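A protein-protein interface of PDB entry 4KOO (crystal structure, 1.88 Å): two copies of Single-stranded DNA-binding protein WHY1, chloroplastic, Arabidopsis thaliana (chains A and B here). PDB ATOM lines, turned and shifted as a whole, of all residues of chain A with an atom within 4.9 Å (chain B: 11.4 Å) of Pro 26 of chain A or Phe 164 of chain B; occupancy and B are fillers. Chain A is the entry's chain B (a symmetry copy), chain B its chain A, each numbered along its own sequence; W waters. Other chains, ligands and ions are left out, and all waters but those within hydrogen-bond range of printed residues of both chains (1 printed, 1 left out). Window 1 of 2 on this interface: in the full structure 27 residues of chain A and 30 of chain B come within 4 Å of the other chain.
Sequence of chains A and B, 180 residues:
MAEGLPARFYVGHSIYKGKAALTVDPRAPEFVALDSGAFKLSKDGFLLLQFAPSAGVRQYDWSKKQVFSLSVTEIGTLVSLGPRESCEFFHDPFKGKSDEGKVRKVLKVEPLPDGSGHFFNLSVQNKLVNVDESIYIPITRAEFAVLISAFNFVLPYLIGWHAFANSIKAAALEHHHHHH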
ATOM      1  N   PHE A   9     -28.983 -25.276  20.273  1.00  0.00           N
ATOM      2  CA  PHE A   9     -28.046 -24.235  20.687  1.00  0.00           C
ATOM      3  C   PHE A   9     -28.580 -23.347  21.806  1.00  0.00           C
ATOM      4  O   PHE A   9     -29.702 -22.883  21.747  1.00  0.00           O
ATOM      5  CB  PHE A   9     -27.723 -23.340  19.488  1.00  0.00           C
ATOM      6  CG  PHE A   9     -26.932 -24.029  18.421  1.00  0.00           C
ATOM      7  CD1 PHE A   9     -25.579 -24.246  18.587  1.00  0.00           C
ATOM      8  CD2 PHE A   9     -27.543 -24.475  17.259  1.00  0.00           C
ATOM      9  CE1 PHE A   9     -24.842 -24.897  17.611  1.00  0.00           C
ATOM     10  CE2 PHE A   9     -26.811 -25.125  16.286  1.00  0.00           C
ATOM     11  CZ  PHE A   9     -25.455 -25.334  16.466  1.00  0.00           C
ATOM     12  N   VAL A  11     -27.838 -19.802  23.135  1.00  0.00           N
ATOM     13  CA  VAL A  11     -27.115 -18.631  22.665  1.00  0.00           C
ATOM     14  C   VAL A  11     -27.646 -17.360  23.315  1.00  0.00           C
ATOM     15  O   VAL A  11     -27.616 -16.280  22.714  1.00  0.00           O
ATOM     16  CB  VAL A  11     -27.175 -18.503  21.114  1.00  0.00           C
ATOM     17  CG1 VAL A  11     -26.439 -19.629  20.454  1.00  0.00           C
ATOM     18  CG2 VAL A  11     -28.601 -18.407  20.618  1.00  0.00           C
ATOM     19  N   GLY A  12     -28.071 -17.465  24.571  1.00  0.00           N
ATOM     20  CA  GLY A  12     -28.371 -16.273  25.344  1.00  0.00           C
ATOM     21  C   GLY A  12     -27.357 -15.155  25.208  1.00  0.00           C
ATOM     22  O   GLY A  12     -26.165 -15.368  25.279  1.00  0.00           O
ATOM     23  N   VAL A  24     -30.878 -12.252  27.085  1.00  0.00           N
ATOM     24  CA  VAL A  24     -31.884 -12.348  26.047  1.00  0.00           C
ATOM     25  C   VAL A  24     -31.666 -13.643  25.270  1.00  0.00           C
ATOM     26  O   VAL A  24     -30.585 -13.886  24.697  1.00  0.00           O
ATOM     27  CB  VAL A  24     -31.803 -11.135  25.087  1.00  0.00           C
ATOM     28  CG1 VAL A  24     -32.975 -11.172  24.134  1.00  0.00           C
ATOM     29  CG2 VAL A  24     -31.834  -9.864  25.900  1.00  0.00           C
ATOM     30  N   ASP A  25     -32.702 -14.473  25.292  1.00  0.00           N
ATOM     31  CA  ASP A  25     -32.670 -15.796  24.676  1.00  0.00           C
ATOM     32  C   ASP A  25     -33.742 -15.907  23.607  1.00  0.00           C
ATOM     33  O   ASP A  25     -34.924 -15.769  23.896  1.00  0.00           O
ATOM     34  CB  ASP A  25     -32.937 -16.890  25.714  1.00  0.00           C
ATOM     35  CG  ASP A  25     -31.692 -17.397  26.320  1.00  0.00           C
ATOM     36  OD1 ASP A  25     -31.109 -18.325  25.736  1.00  0.00           O
ATOM     37  OD2 ASP A  25     -31.269 -16.837  27.355  1.00  0.00           O
ATOM     38  N   PRO A  26     -33.326 -16.197  22.378  1.00  0.00           N
ATOM     39  CA  PRO A  26     -34.334 -16.440  21.338  1.00  0.00           C
ATOM     40  C   PRO A  26     -35.063 -17.771  21.501  1.00  0.00           C
ATOM     41  O   PRO A  26     -34.461 -18.742  21.926  1.00  0.00           O
ATOM     42  CB  PRO A  26     -33.501 -16.375  20.060  1.00  0.00           C
ATOM     43  CG  PRO A  26     -32.132 -16.736  20.426  1.00  0.00           C
ATOM     44  CD  PRO A  26     -31.946 -16.331  21.876  1.00  0.00           C
ATOM     45  N   ARG A  27     -36.347 -17.797  21.189  1.00  0.00           N
ATOM     46  CA  ARG A  27     -37.153 -19.004  21.248  1.00  0.00           C
ATOM     47  C   ARG A  27     -37.832 -19.233  19.922  1.00  0.00           C
ATOM     48  O   ARG A  27     -38.459 -18.339  19.350  1.00  0.00           O
ATOM     49  CB  ARG A  27     -38.197 -18.918  22.363  1.00  0.00           C
ATOM     50  CG  ARG A  27     -37.603 -18.807  23.738  1.00  0.00           C
ATOM     51  CD  ARG A  27     -36.989 -20.167  24.093  1.00  0.00           C
ATOM     52  NE  ARG A  27     -36.134 -20.109  25.273  1.00  0.00           N
ATOM     53  CZ  ARG A  27     -36.574 -20.245  26.515  1.00  0.00           C
ATOM     54  NH1 ARG A  27     -37.879 -20.440  26.748  1.00  0.00           N
ATOM     55  NH2 ARG A  27     -35.708 -20.178  27.528  1.00  0.00           N
ATOM     56  N   ALA A  28     -37.725 -20.466  19.443  1.00  0.00           N
ATOM     57  CA  ALA A  28     -38.212 -20.804  18.113  1.00  0.00           C
ATOM     58  C   ALA A  28     -39.725 -20.801  18.027  1.00  0.00           C
ATOM     59  O   ALA A  28     -40.444 -21.012  19.027  1.00  0.00           O
ATOM     60  CB  ALA A  28     -37.637 -22.207  17.703  1.00  0.00           C
ATOM     61  N   PHE A  46     -40.379 -15.935  19.870  1.00  0.00           N
ATOM     62  CA  PHE A  46     -40.348 -14.777  20.737  1.00  0.00           C
ATOM     63  C   PHE A  46     -38.985 -14.692  21.371  1.00  0.00           C
ATOM     64  O   PHE A  46     -38.136 -15.591  21.176  1.00  0.00           O
ATOM     65  CB  PHE A  46     -41.466 -14.844  21.794  1.00  0.00           C
ATOM     66  CG  PHE A  46     -41.328 -16.009  22.766  1.00  0.00           C
ATOM     67  CD1 PHE A  46     -41.819 -17.267  22.432  1.00  0.00           C
ATOM     68  CD2 PHE A  46     -40.734 -15.833  23.993  1.00  0.00           C
ATOM     69  CE1 PHE A  46     -41.702 -18.335  23.333  1.00  0.00           C
ATOM     70  CE2 PHE A  46     -40.611 -16.900  24.886  1.00  0.00           C
ATOM     71  CZ  PHE A  46     -41.095 -18.135  24.544  1.00  0.00           C
ATOM     72  N   LEU A  47     -38.754 -13.618  22.128  1.00  0.00           N
ATOM     73  CA  LEU A  47     -37.512 -13.468  22.851  1.00  0.00           C
ATOM     74  C   LEU A  47     -37.799 -13.499  24.344  1.00  0.00           C
ATOM     75  O   LEU A  47     -38.675 -12.818  24.826  1.00  0.00           O
ATOM     76  CB  LEU A  47     -36.795 -12.176  22.524  1.00  0.00           C
ATOM     77  CG  LEU A  47     -36.446 -11.955  21.046  1.00  0.00           C
ATOM     78  CD1 LEU A  47     -35.781 -10.617  20.873  1.00  0.00           C
ATOM     79  CD2 LEU A  47     -35.581 -13.077  20.565  1.00  0.00           C
ATOM     80  N   VAL A 154     -33.405 -11.252  13.895  1.00  0.00           N
ATOM     81  CA  VAL A 154     -34.127 -12.450  14.287  1.00  0.00           C
ATOM     82  C   VAL A 154     -35.608 -12.455  13.889  1.00  0.00           C
ATOM     83  O   VAL A 154     -36.222 -13.503  13.710  1.00  0.00           O
ATOM     84  CB  VAL A 154     -33.944 -12.727  15.794  1.00  0.00           C
ATOM     85  CG1 VAL A 154     -34.948 -11.983  16.625  1.00  0.00           C
ATOM     86  CG2 VAL A 154     -34.060 -14.206  16.044  1.00  0.00           C
ATOM     87  N   LEU A 158     -38.419 -15.652  13.522  1.00  0.00           N
ATOM     88  CA  LEU A 158     -39.440 -15.897  14.514  1.00  0.00           C
ATOM     89  C   LEU A 158     -40.784 -16.152  13.878  1.00  0.00           C
ATOM     90  O   LEU A 158     -41.620 -16.822  14.465  1.00  0.00           O
ATOM     91  CB  LEU A 158     -39.537 -14.764  15.502  1.00  0.00           C
ATOM     92  CG  LEU A 158     -38.279 -14.516  16.365  1.00  0.00           C
ATOM     93  CD1 LEU A 158     -38.538 -13.378  17.306  1.00  0.00           C
ATOM     94  CD2 LEU A 158     -37.795 -15.768  17.119  1.00  0.00           C
ATOM     95  N   PRO B  29     -17.637 -17.381  17.051  1.00  0.00           N
ATOM     96  CA  PRO B  29     -17.934 -17.655  18.433  1.00  0.00           C
ATOM     97  C   PRO B  29     -17.489 -19.093  18.765  1.00  0.00           C
ATOM     98  O   PRO B  29     -17.376 -19.877  17.840  1.00  0.00           O
ATOM     99  CB  PRO B  29     -19.443 -17.566  18.476  1.00  0.00           C
ATOM    100  CG  PRO B  29     -19.891 -17.821  17.114  1.00  0.00           C
ATOM    101  CD  PRO B  29     -18.861 -17.271  16.225  1.00  0.00           C
ATOM    102  N   PHE B  31     -18.391 -22.579  21.138  1.00  0.00           N
ATOM    103  CA  PHE B  31     -19.449 -23.283  21.845  1.00  0.00           C
ATOM    104  C   PHE B  31     -18.847 -24.470  22.622  1.00  0.00           C
ATOM    105  O   PHE B  31     -17.748 -24.934  22.323  1.00  0.00           O
ATOM    106  CB  PHE B  31     -20.457 -23.857  20.869  1.00  0.00           C
ATOM    107  CG  PHE B  31     -21.268 -22.829  20.146  1.00  0.00           C
ATOM    108  CD1 PHE B  31     -20.789 -22.238  18.994  1.00  0.00           C
ATOM    109  CD2 PHE B  31     -22.517 -22.468  20.607  1.00  0.00           C
ATOM    110  CE1 PHE B  31     -21.540 -21.303  18.325  1.00  0.00           C
ATOM    111  CE2 PHE B  31     -23.280 -21.542  19.924  1.00  0.00           C
ATOM    112  CZ  PHE B  31     -22.783 -20.953  18.798  1.00  0.00           C
ATOM    113  N   PHE B  39     -25.500 -27.522  22.707  1.00  0.00           N
ATOM    114  CA  PHE B  39     -24.313 -26.689  22.582  1.00  0.00           C
ATOM    115  C   PHE B  39     -24.572 -25.317  23.184  1.00  0.00           C
ATOM    116  O   PHE B  39     -25.518 -24.683  22.799  1.00  0.00           O
ATOM    117  CB  PHE B  39     -23.979 -26.535  21.107  1.00  0.00           C
ATOM    118  CG  PHE B  39     -23.400 -27.770  20.487  1.00  0.00           C
ATOM    119  CD1 PHE B  39     -22.334 -28.422  21.084  1.00  0.00           C
ATOM    120  CD2 PHE B  39     -23.914 -28.272  19.303  1.00  0.00           C
ATOM    121  CE1 PHE B  39     -21.791 -29.553  20.509  1.00  0.00           C
ATOM    122  CE2 PHE B  39     -23.372 -29.403  18.722  1.00  0.00           C
ATOM    123  CZ  PHE B  39     -22.314 -30.042  19.324  1.00  0.00           C
ATOM    124  N   LYS B  40     -23.754 -24.885  24.140  1.00  0.00           N
ATOM    125  CA  LYS B  40     -23.936 -23.583  24.764  1.00  0.00           C
ATOM    126  C   LYS B  40     -22.879 -22.625  24.258  1.00  0.00           C
ATOM    127  O   LYS B  40     -21.711 -22.985  24.140  1.00  0.00           O
ATOM    128  CB  LYS B  40     -23.837 -23.688  26.283  1.00  0.00           C
ATOM    129  CG  LYS B  40     -24.208 -22.421  27.022  1.00  0.00           C
ATOM    130  CD  LYS B  40     -24.024 -22.574  28.534  1.00  0.00           C
ATOM    131  CE  LYS B  40     -24.208 -21.261  29.274  1.00  0.00           C
ATOM    132  NZ  LYS B  40     -25.630 -20.809  29.284  1.00  0.00           N
ATOM    133  N   LEU B  41     -23.285 -21.389  23.971  1.00  0.00           N
ATOM    134  CA  LEU B  41     -22.337 -20.369  23.582  1.00  0.00           C
ATOM    135  C   LEU B  41     -21.386 -20.103  24.747  1.00  0.00           C
ATOM    136  O   LEU B  41     -21.843 -19.807  25.831  1.00  0.00           O
ATOM    137  CB  LEU B  41     -23.083 -19.069  23.242  1.00  0.00           C
ATOM    138  CG  LEU B  41     -22.224 -17.864  22.936  1.00  0.00           C
ATOM    139  CD1 LEU B  41     -21.459 -18.065  21.683  1.00  0.00           C
ATOM    140  CD2 LEU B  41     -23.157 -16.636  22.834  1.00  0.00           C
ATOM    141  N   ASP B  44     -18.287 -15.100  22.683  1.00  0.00           N
ATOM    142  CA  ASP B  44     -18.656 -14.375  21.439  1.00  0.00           C
ATOM    143  C   ASP B  44     -17.518 -14.371  20.426  1.00  0.00           C
ATOM    144  O   ASP B  44     -16.323 -14.380  20.758  1.00  0.00           O
ATOM    145  CB  ASP B  44     -19.030 -12.899  21.722  1.00  0.00           C
ATOM    146  CG  ASP B  44     -20.348 -12.741  22.462  1.00  0.00           C
ATOM    147  OD1 ASP B  44     -21.118 -13.720  22.576  1.00  0.00           O
ATOM    148  OD2 ASP B  44     -20.621 -11.588  22.930  1.00  0.00           O
ATOM    149  N   LEU B 155     -22.630  -9.281  12.967  1.00  0.00           N
ATOM    150  CA  LEU B 155     -22.996  -9.129  14.371  1.00  0.00           C
ATOM    151  C   LEU B 155     -23.855 -10.294  14.905  1.00  0.00           C
ATOM    152  O   LEU B 155     -23.513 -10.891  15.916  1.00  0.00           O
ATOM    153  CB  LEU B 155     -23.628  -7.756  14.548  1.00  0.00           C
ATOM    154  CG  LEU B 155     -23.571  -6.940  15.835  1.00  0.00           C
ATOM    155  CD1 LEU B 155     -22.291  -7.068  16.557  1.00  0.00           C
ATOM    156  CD2 LEU B 155     -23.830  -5.469  15.507  1.00  0.00           C
ATOM    157  N   PRO B 156     -24.967 -10.648  14.233  1.00  0.00           N
ATOM    158  CA  PRO B 156     -25.725 -11.813  14.755  1.00  0.00           C
ATOM    159  C   PRO B 156     -24.977 -13.135  14.715  1.00  0.00           C
ATOM    160  O   PRO B 156     -25.313 -13.997  15.535  1.00  0.00           O
ATOM    161  CB  PRO B 156     -26.937 -11.914  13.826  1.00  0.00           C
ATOM    162  CG  PRO B 156     -27.031 -10.539  13.202  1.00  0.00           C
ATOM    163  CD  PRO B 156     -25.658  -9.999  13.102  1.00  0.00           C
ATOM    164  N   TYR B 157     -24.010 -13.292  13.805  1.00  0.00           N
ATOM    165  CA  TYR B 157     -23.194 -14.483  13.779  1.00  0.00           C
ATOM    166  C   TYR B 157     -22.297 -14.507  14.989  1.00  0.00           C
ATOM    167  O   TYR B 157     -22.063 -15.571  15.544  1.00  0.00           O
ATOM    168  CB  TYR B 157     -22.282 -14.564  12.560  1.00  0.00           C
ATOM    169  CG  TYR B 157     -22.979 -14.917  11.279  1.00  0.00           C
ATOM    170  CD1 TYR B 157     -23.889 -14.062  10.679  1.00  0.00           C
ATOM    171  CD2 TYR B 157     -22.667 -16.110  10.635  1.00  0.00           C
ATOM    172  CE1 TYR B 157     -24.525 -14.430   9.478  1.00  0.00           C
ATOM    173  CE2 TYR B 157     -23.258 -16.462   9.459  1.00  0.00           C
ATOM    174  CZ  TYR B 157     -24.187 -15.640   8.882  1.00  0.00           C
ATOM    175  OH  TYR B 157     -24.749 -16.077   7.689  1.00  0.00           O
ATOM    176  N   LEU B 158     -21.725 -13.361  15.342  1.00  0.00           N
ATOM    177  CA  LEU B 158     -20.757 -13.320  16.439  1.00  0.00           C
ATOM    178  C   LEU B 158     -21.346 -13.670  17.808  1.00  0.00           C
ATOM    179  O   LEU B 158     -20.600 -14.076  18.720  1.00  0.00           O
ATOM    180  CB  LEU B 158     -20.064 -11.957  16.499  1.00  0.00           C
ATOM    181  CG  LEU B 158     -19.259 -11.494  15.281  1.00  0.00           C
ATOM    182  CD1 LEU B 158     -18.559 -10.190  15.591  1.00  0.00           C
ATOM    183  CD2 LEU B 158     -18.270 -12.545  14.745  1.00  0.00           C
ATOM    184  N   ILE B 159     -22.648 -13.471  17.957  1.00  0.00           N
ATOM    185  CA  ILE B 159     -23.361 -13.794  19.181  1.00  0.00           C
ATOM    186  C   ILE B 159     -24.108 -15.124  19.107  1.00  0.00           C
ATOM    187  O   ILE B 159     -24.848 -15.486  20.038  1.00  0.00           O
ATOM    188  CB  ILE B 159     -24.286 -12.655  19.660  1.00  0.00           C
ATOM    189  CG1 ILE B 159     -25.456 -12.466  18.710  1.00  0.00           C
ATOM    190  CG2 ILE B 159     -23.491 -11.353  19.920  1.00  0.00           C
ATOM    191  CD1 ILE B 159     -26.584 -11.627  19.285  1.00  0.00           C
ATOM    192  N   GLY B 160     -23.922 -15.842  18.005  1.00  0.00           N
ATOM    193  CA  GLY B 160     -24.459 -17.187  17.892  1.00  0.00           C
ATOM    194  C   GLY B 160     -25.879 -17.294  17.411  1.00  0.00           C
ATOM    195  O   GLY B 160     -26.456 -18.388  17.349  1.00  0.00           O
ATOM    196  N   TRP B 161     -26.482 -16.156  17.096  1.00  0.00           N
ATOM    197  CA  TRP B 161     -27.903 -16.162  16.783  1.00  0.00           C
ATOM    198  C   TRP B 161     -28.202 -16.762  15.405  1.00  0.00           C
ATOM    199  O   TRP B 161     -29.325 -17.192  15.119  1.00  0.00           O
ATOM    200  CB  TRP B 161     -28.529 -14.781  16.977  1.00  0.00           C
ATOM    201  CG  TRP B 161     -28.850 -14.461  18.435  1.00  0.00           C
ATOM    202  CD1 TRP B 161     -28.189 -14.935  19.546  1.00  0.00           C
ATOM    203  CD2 TRP B 161     -29.895 -13.613  18.929  1.00  0.00           C
ATOM    204  NE1 TRP B 161     -28.744 -14.418  20.681  1.00  0.00           N
ATOM    205  CE2 TRP B 161     -29.807 -13.623  20.339  1.00  0.00           C
ATOM    206  CE3 TRP B 161     -30.890 -12.830  18.320  1.00  0.00           C
ATOM    207  CZ2 TRP B 161     -30.680 -12.901  21.139  1.00  0.00           C
ATOM    208  CZ3 TRP B 161     -31.771 -12.122  19.114  1.00  0.00           C
ATOM    209  CH2 TRP B 161     -31.670 -12.157  20.510  1.00  0.00           C
ATOM    210  N   HIS B 162     -27.191 -16.767  14.550  1.00  0.00           N
ATOM    211  CA  HIS B 162     -27.231 -17.470  13.269  1.00  0.00           C
ATOM    212  C   HIS B 162     -27.441 -18.942  13.457  1.00  0.00           C
ATOM    213  O   HIS B 162     -28.212 -19.596  12.733  1.00  0.00           O
ATOM    214  CB  HIS B 162     -25.887 -17.286  12.558  1.00  0.00           C
ATOM    215  CG  HIS B 162     -24.751 -18.081  13.154  1.00  0.00           C
ATOM    216  ND1 HIS B 162     -24.205 -17.823  14.403  1.00  0.00           N
ATOM    217  CD2 HIS B 162     -24.033 -19.112  12.636  1.00  0.00           C
ATOM    218  CE1 HIS B 162     -23.210 -18.661  14.616  1.00  0.00           C
ATOM    219  NE2 HIS B 162     -23.088 -19.452  13.560  1.00  0.00           N
ATOM    220  N   ALA B 163     -26.724 -19.477  14.446  1.00  0.00           N
ATOM    221  CA  ALA B 163     -26.756 -20.885  14.746  1.00  0.00           C
ATOM    222  C   ALA B 163     -28.128 -21.217  15.254  1.00  0.00           C
ATOM    223  O   ALA B 163     -28.687 -22.244  14.877  1.00  0.00           O
ATOM    224  CB  ALA B 163     -25.685 -21.252  15.791  1.00  0.00           C
ATOM    225  N   PHE B 164     -28.706 -20.329  16.061  1.00  0.00           N
ATOM    226  CA  PHE B 164     -30.096 -20.502  16.479  1.00  0.00           C
ATOM    227  C   PHE B 164     -31.020 -20.473  15.295  1.00  0.00           C
ATOM    228  O   PHE B 164     -31.900 -21.365  15.118  1.00  0.00           O
ATOM    229  CB  PHE B 164     -30.537 -19.428  17.488  1.00  0.00           C
ATOM    230  CG  PHE B 164     -32.042 -19.197  17.527  1.00  0.00           C
ATOM    231  CD1 PHE B 164     -32.876 -19.995  18.291  1.00  0.00           C
ATOM    232  CD2 PHE B 164     -32.614 -18.211  16.799  1.00  0.00           C
ATOM    233  CE1 PHE B 164     -34.243 -19.779  18.316  1.00  0.00           C
ATOM    234  CE2 PHE B 164     -33.993 -17.979  16.825  1.00  0.00           C
ATOM    235  CZ  PHE B 164     -34.807 -18.771  17.602  1.00  0.00           C
ATOM    236  N   ALA B 165     -30.851 -19.440  14.471  1.00  0.00           N
ATOM    237  CA  ALA B 165     -31.793 -19.202  13.381  1.00  0.00           C
ATOM    238  C   ALA B 165     -31.805 -20.375  12.432  1.00  0.00           C
ATOM    239  O   ALA B 165     -32.857 -20.763  11.904  1.00  0.00           O
ATOM    240  CB  ALA B 165     -31.435 -17.897  12.579  1.00  0.00           C
ATOM    241  N   ASN B 166     -30.626 -20.931  12.212  1.00  0.00           N
ATOM    242  CA  ASN B 166     -30.478 -21.963  11.209  1.00  0.00           C
ATOM    243  C   ASN B 166     -30.753 -23.369  11.736  1.00  0.00           C
ATOM    244  O   ASN B 166     -30.711 -24.339  10.967  1.00  0.00           O
ATOM    245  CB  ASN B 166     -29.081 -21.847  10.554  1.00  0.00           C
ATOM    246  CG  ASN B 166     -29.039 -20.763   9.495  1.00  0.00           C
ATOM    247  OD1 ASN B 166     -28.887 -19.578   9.806  1.00  0.00           O
ATOM    248  ND2 ASN B 166     -29.207 -21.157   8.231  1.00  0.00           N
ATOM    249  N   SER B 167     -31.082 -23.471  13.020  1.00  0.00           N
ATOM    250  CA  SER B 167     -31.426 -24.730  13.648  1.00  0.00           C
ATOM    251  C   SER B 167     -32.931 -24.903  13.736  1.00  0.00           C
ATOM    252  O   SER B 167     -33.419 -25.952  14.195  1.00  0.00           O
ATOM    253  CB  SER B 167     -30.856 -24.791  15.049  1.00  0.00           C
ATOM    254  OG  SER B 167     -31.634 -23.993  15.942  1.00  0.00           O
ATOM    255  N   ILE B 168     -33.669 -23.877  13.319  1.00  0.00           N
ATOM    256  CA  ILE B 168     -35.119 -23.873  13.519  1.00  0.00           C
ATOM    257  C   ILE B 168     -35.792 -24.972  12.669  1.00  0.00           C
ATOM    258  O   ILE B 168     -36.564 -25.753  13.193  1.00  0.00           O
ATOM    259  CB  ILE B 168     -35.772 -22.495  13.201  1.00  0.00           C
ATOM    260  CG1 ILE B 168     -35.404 -21.429  14.252  1.00  0.00           C
ATOM    261  CG2 ILE B 168     -37.266 -22.613  13.155  1.00  0.00           C
ATOM    262  CD1 ILE B 168     -35.888 -19.962  13.845  1.00  0.00           C
ATOM    263  N   LYS B 169     -35.519 -24.980  11.368  1.00  0.00           N
ATOM    264  CA  LYS B 169     -36.193 -25.908  10.458  1.00  0.00           C
ATOM    265  C   LYS B 169     -35.924 -27.321  10.922  1.00  0.00           C
ATOM    266  O   LYS B 169     -36.844 -28.110  11.141  1.00  0.00           O
ATOM    267  CB  LYS B 169     -35.669 -25.782   9.035  1.00  0.00           C
ATOM    268  CG  LYS B 169     -36.121 -24.603   8.227  1.00  0.00           C
ATOM    269  CD  LYS B 169     -35.470 -24.684   6.825  1.00  0.00           C
ATOM    270  CE  LYS B 169     -35.335 -23.320   6.171  1.00  0.00           C
ATOM    271  NZ  LYS B 169     -34.412 -23.250   4.996  1.00  0.00           N
ATOM    272  N   ALA B 170     -34.643 -27.639  11.079  1.00  0.00           N
ATOM    273  CA  ALA B 170     -34.260 -29.016  11.330  1.00  0.00           C
ATOM    274  C   ALA B 170     -34.927 -29.445  12.623  1.00  0.00           C
ATOM    275  O   ALA B 170     -35.416 -30.570  12.722  1.00  0.00           O
ATOM    276  CB  ALA B 170     -32.742 -29.169  11.392  1.00  0.00           C
ATOM    277  N   ALA B 171     -35.001 -28.527  13.587  1.00  0.00           N
ATOM    278  CA  ALA B 171     -35.639 -28.814  14.863  1.00  0.00           C
ATOM    279  C   ALA B 171     -37.131 -29.064  14.719  1.00  0.00           C
ATOM    280  O   ALA B 171     -37.674 -29.962  15.373  1.00  0.00           O
ATOM    281  CB  ALA B 171     -35.388 -27.682  15.849  1.00  0.00           C
ATOM    282  N   ALA B 172     -37.806 -28.264  13.891  1.00  0.00           N
ATOM    283  CA  ALA B 172     -39.263 -28.402  13.707  1.00  0.00           C
ATOM    284  C   ALA B 172     -39.604 -29.793  13.159  1.00  0.00           C
ATOM    285  O   ALA B 172     -40.703 -30.301  13.380  1.00  0.00           O
ATOM    286  CB  ALA B 172     -39.778 -27.370  12.725  1.00  0.00           C
HETATM  287  O   HOH W   1     -31.797 -24.060  18.649  1.00  0.00           O
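1 position is printed for both chains. Of the 16 pairs that touch across the chains among the printed residues, none has its exchanged pair printed and touching as well.
Pro 26 of chain A touches just these residues of chain B: Trp 161 and Phe 164. Of chain A, only Val 11, Pro 26, Arg 27, Ala 28 and Val 154 come within 4 Å of Phe 164 of chain B. Of chain B, only Phe 31, Ile 159, Gly 160, Trp 161 and Phe 164 come within 4 Å of Val 11 of chain A. No residue of chain B comes within 4 Å of Gly 12 of chain A. No residue of chain B comes within 4 Å of Asp 25 of chain A. Of the printed residues of chain B, Arg 27 of chain A touches Phe 164. Of the printed residues of chain B, Ala 28 of chain A touches Phe 164. No residue of chain B comes within 4 Å of Phe 46 of chain A. Printed residues of chain A within 4 Å of Phe 39 of chain B: Phe 9 (3.3 Å). Of the printed residues of chain B, Val 24 of chain A touches Trp 161 (3.7 Å). Printed residues of chain A within 4 Å of Gly 160 of chain B: Val 11. The nearest residue of chain A that does not touch Phe 164 of chain B is Leu 158 of chain A (4.3 Å). The nearest printed residue of chain B that does not touch Val 154 of chain A is Ala 165 of chain B (5.7 Å).
NE1 of Trp 161 of chain B is in hydrogen-bond range of O of Val 11 of chain A (3.0 Å).
N of Trp 161 of chain B lies within hydrogen-bond range of O of Pro 156 of chain B (2.9 Å). The backbone carbonyl oxygen of Phe 164 of chain B is in hydrogen-bond range of the side-chain hydroxyl of Ser 167 of chain B, at 2.8 Å. The backbone carbonyl oxygen of Phe 46 of chain A is in hydrogen-bond range of the backbone NH of Arg 27 of chain A, at 2.8 Å.
Of the 12 printed residues of chain A, 7 touch a printed residue of chain B. Along chain A the printed residues that touch a printed residue of chain B span positions 9 to 154. Of the 24 printed residues of chain B, 8 touch a printed residue of chain A. Hydrophobic or aromatic side chains of chain B that line the printed part of chain A: Phe 31, Phe 39, Trp 161, Ala 163 and Phe 164. Among the printed residues, no Asp or Glu carboxylate lies within 4 Å of a Lys or Arg side-chain nitrogen of the other chain.
Among the printed residues, merely in contact across the chains: Phe 9 of chain A with Phe 39 of chain B (3.3 Å), Val 11 of chain A with Gly 160 of chain B (3.3 Å), Phe 9 of chain A with Ala 163 of chain B (3.5 Å), Pro 26 of chain A with Phe 164 of chain B (3.6 Å), Val 24 of chain A with Trp 161 of chain B (3.7 Å), Ala 28 of chain A with Phe 164 of chain B (3.7 Å), Pro 26 of chain A with Trp 161 of chain B (3.7 Å), Val 11 of chain A with Phe 31 of chain B (3.7 Å), Phe 9 of chain A with Phe 31 of chain B (3.8 Å), Val 11 of chain A with Phe 164 of chain B (3.8 Å), Arg 27 of chain A with Phe 164 of chain B (3.8 Å), Val 154 of chain A with Phe 164 of chain B (3.9 Å), Val 11 of chain A with Ile 159 of chain B (3.9 Å), Val 154 of chain A with Trp 161 of chain B (3.96 Å) and Phe 9 of chain A with Ser 167 of chain B (3.99 Å).
Water W1 lies within hydrogen-bond range of OG of Ser 167 of chain B (2.7 Å) and N of Phe 9 of chain A (3.5 Å).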
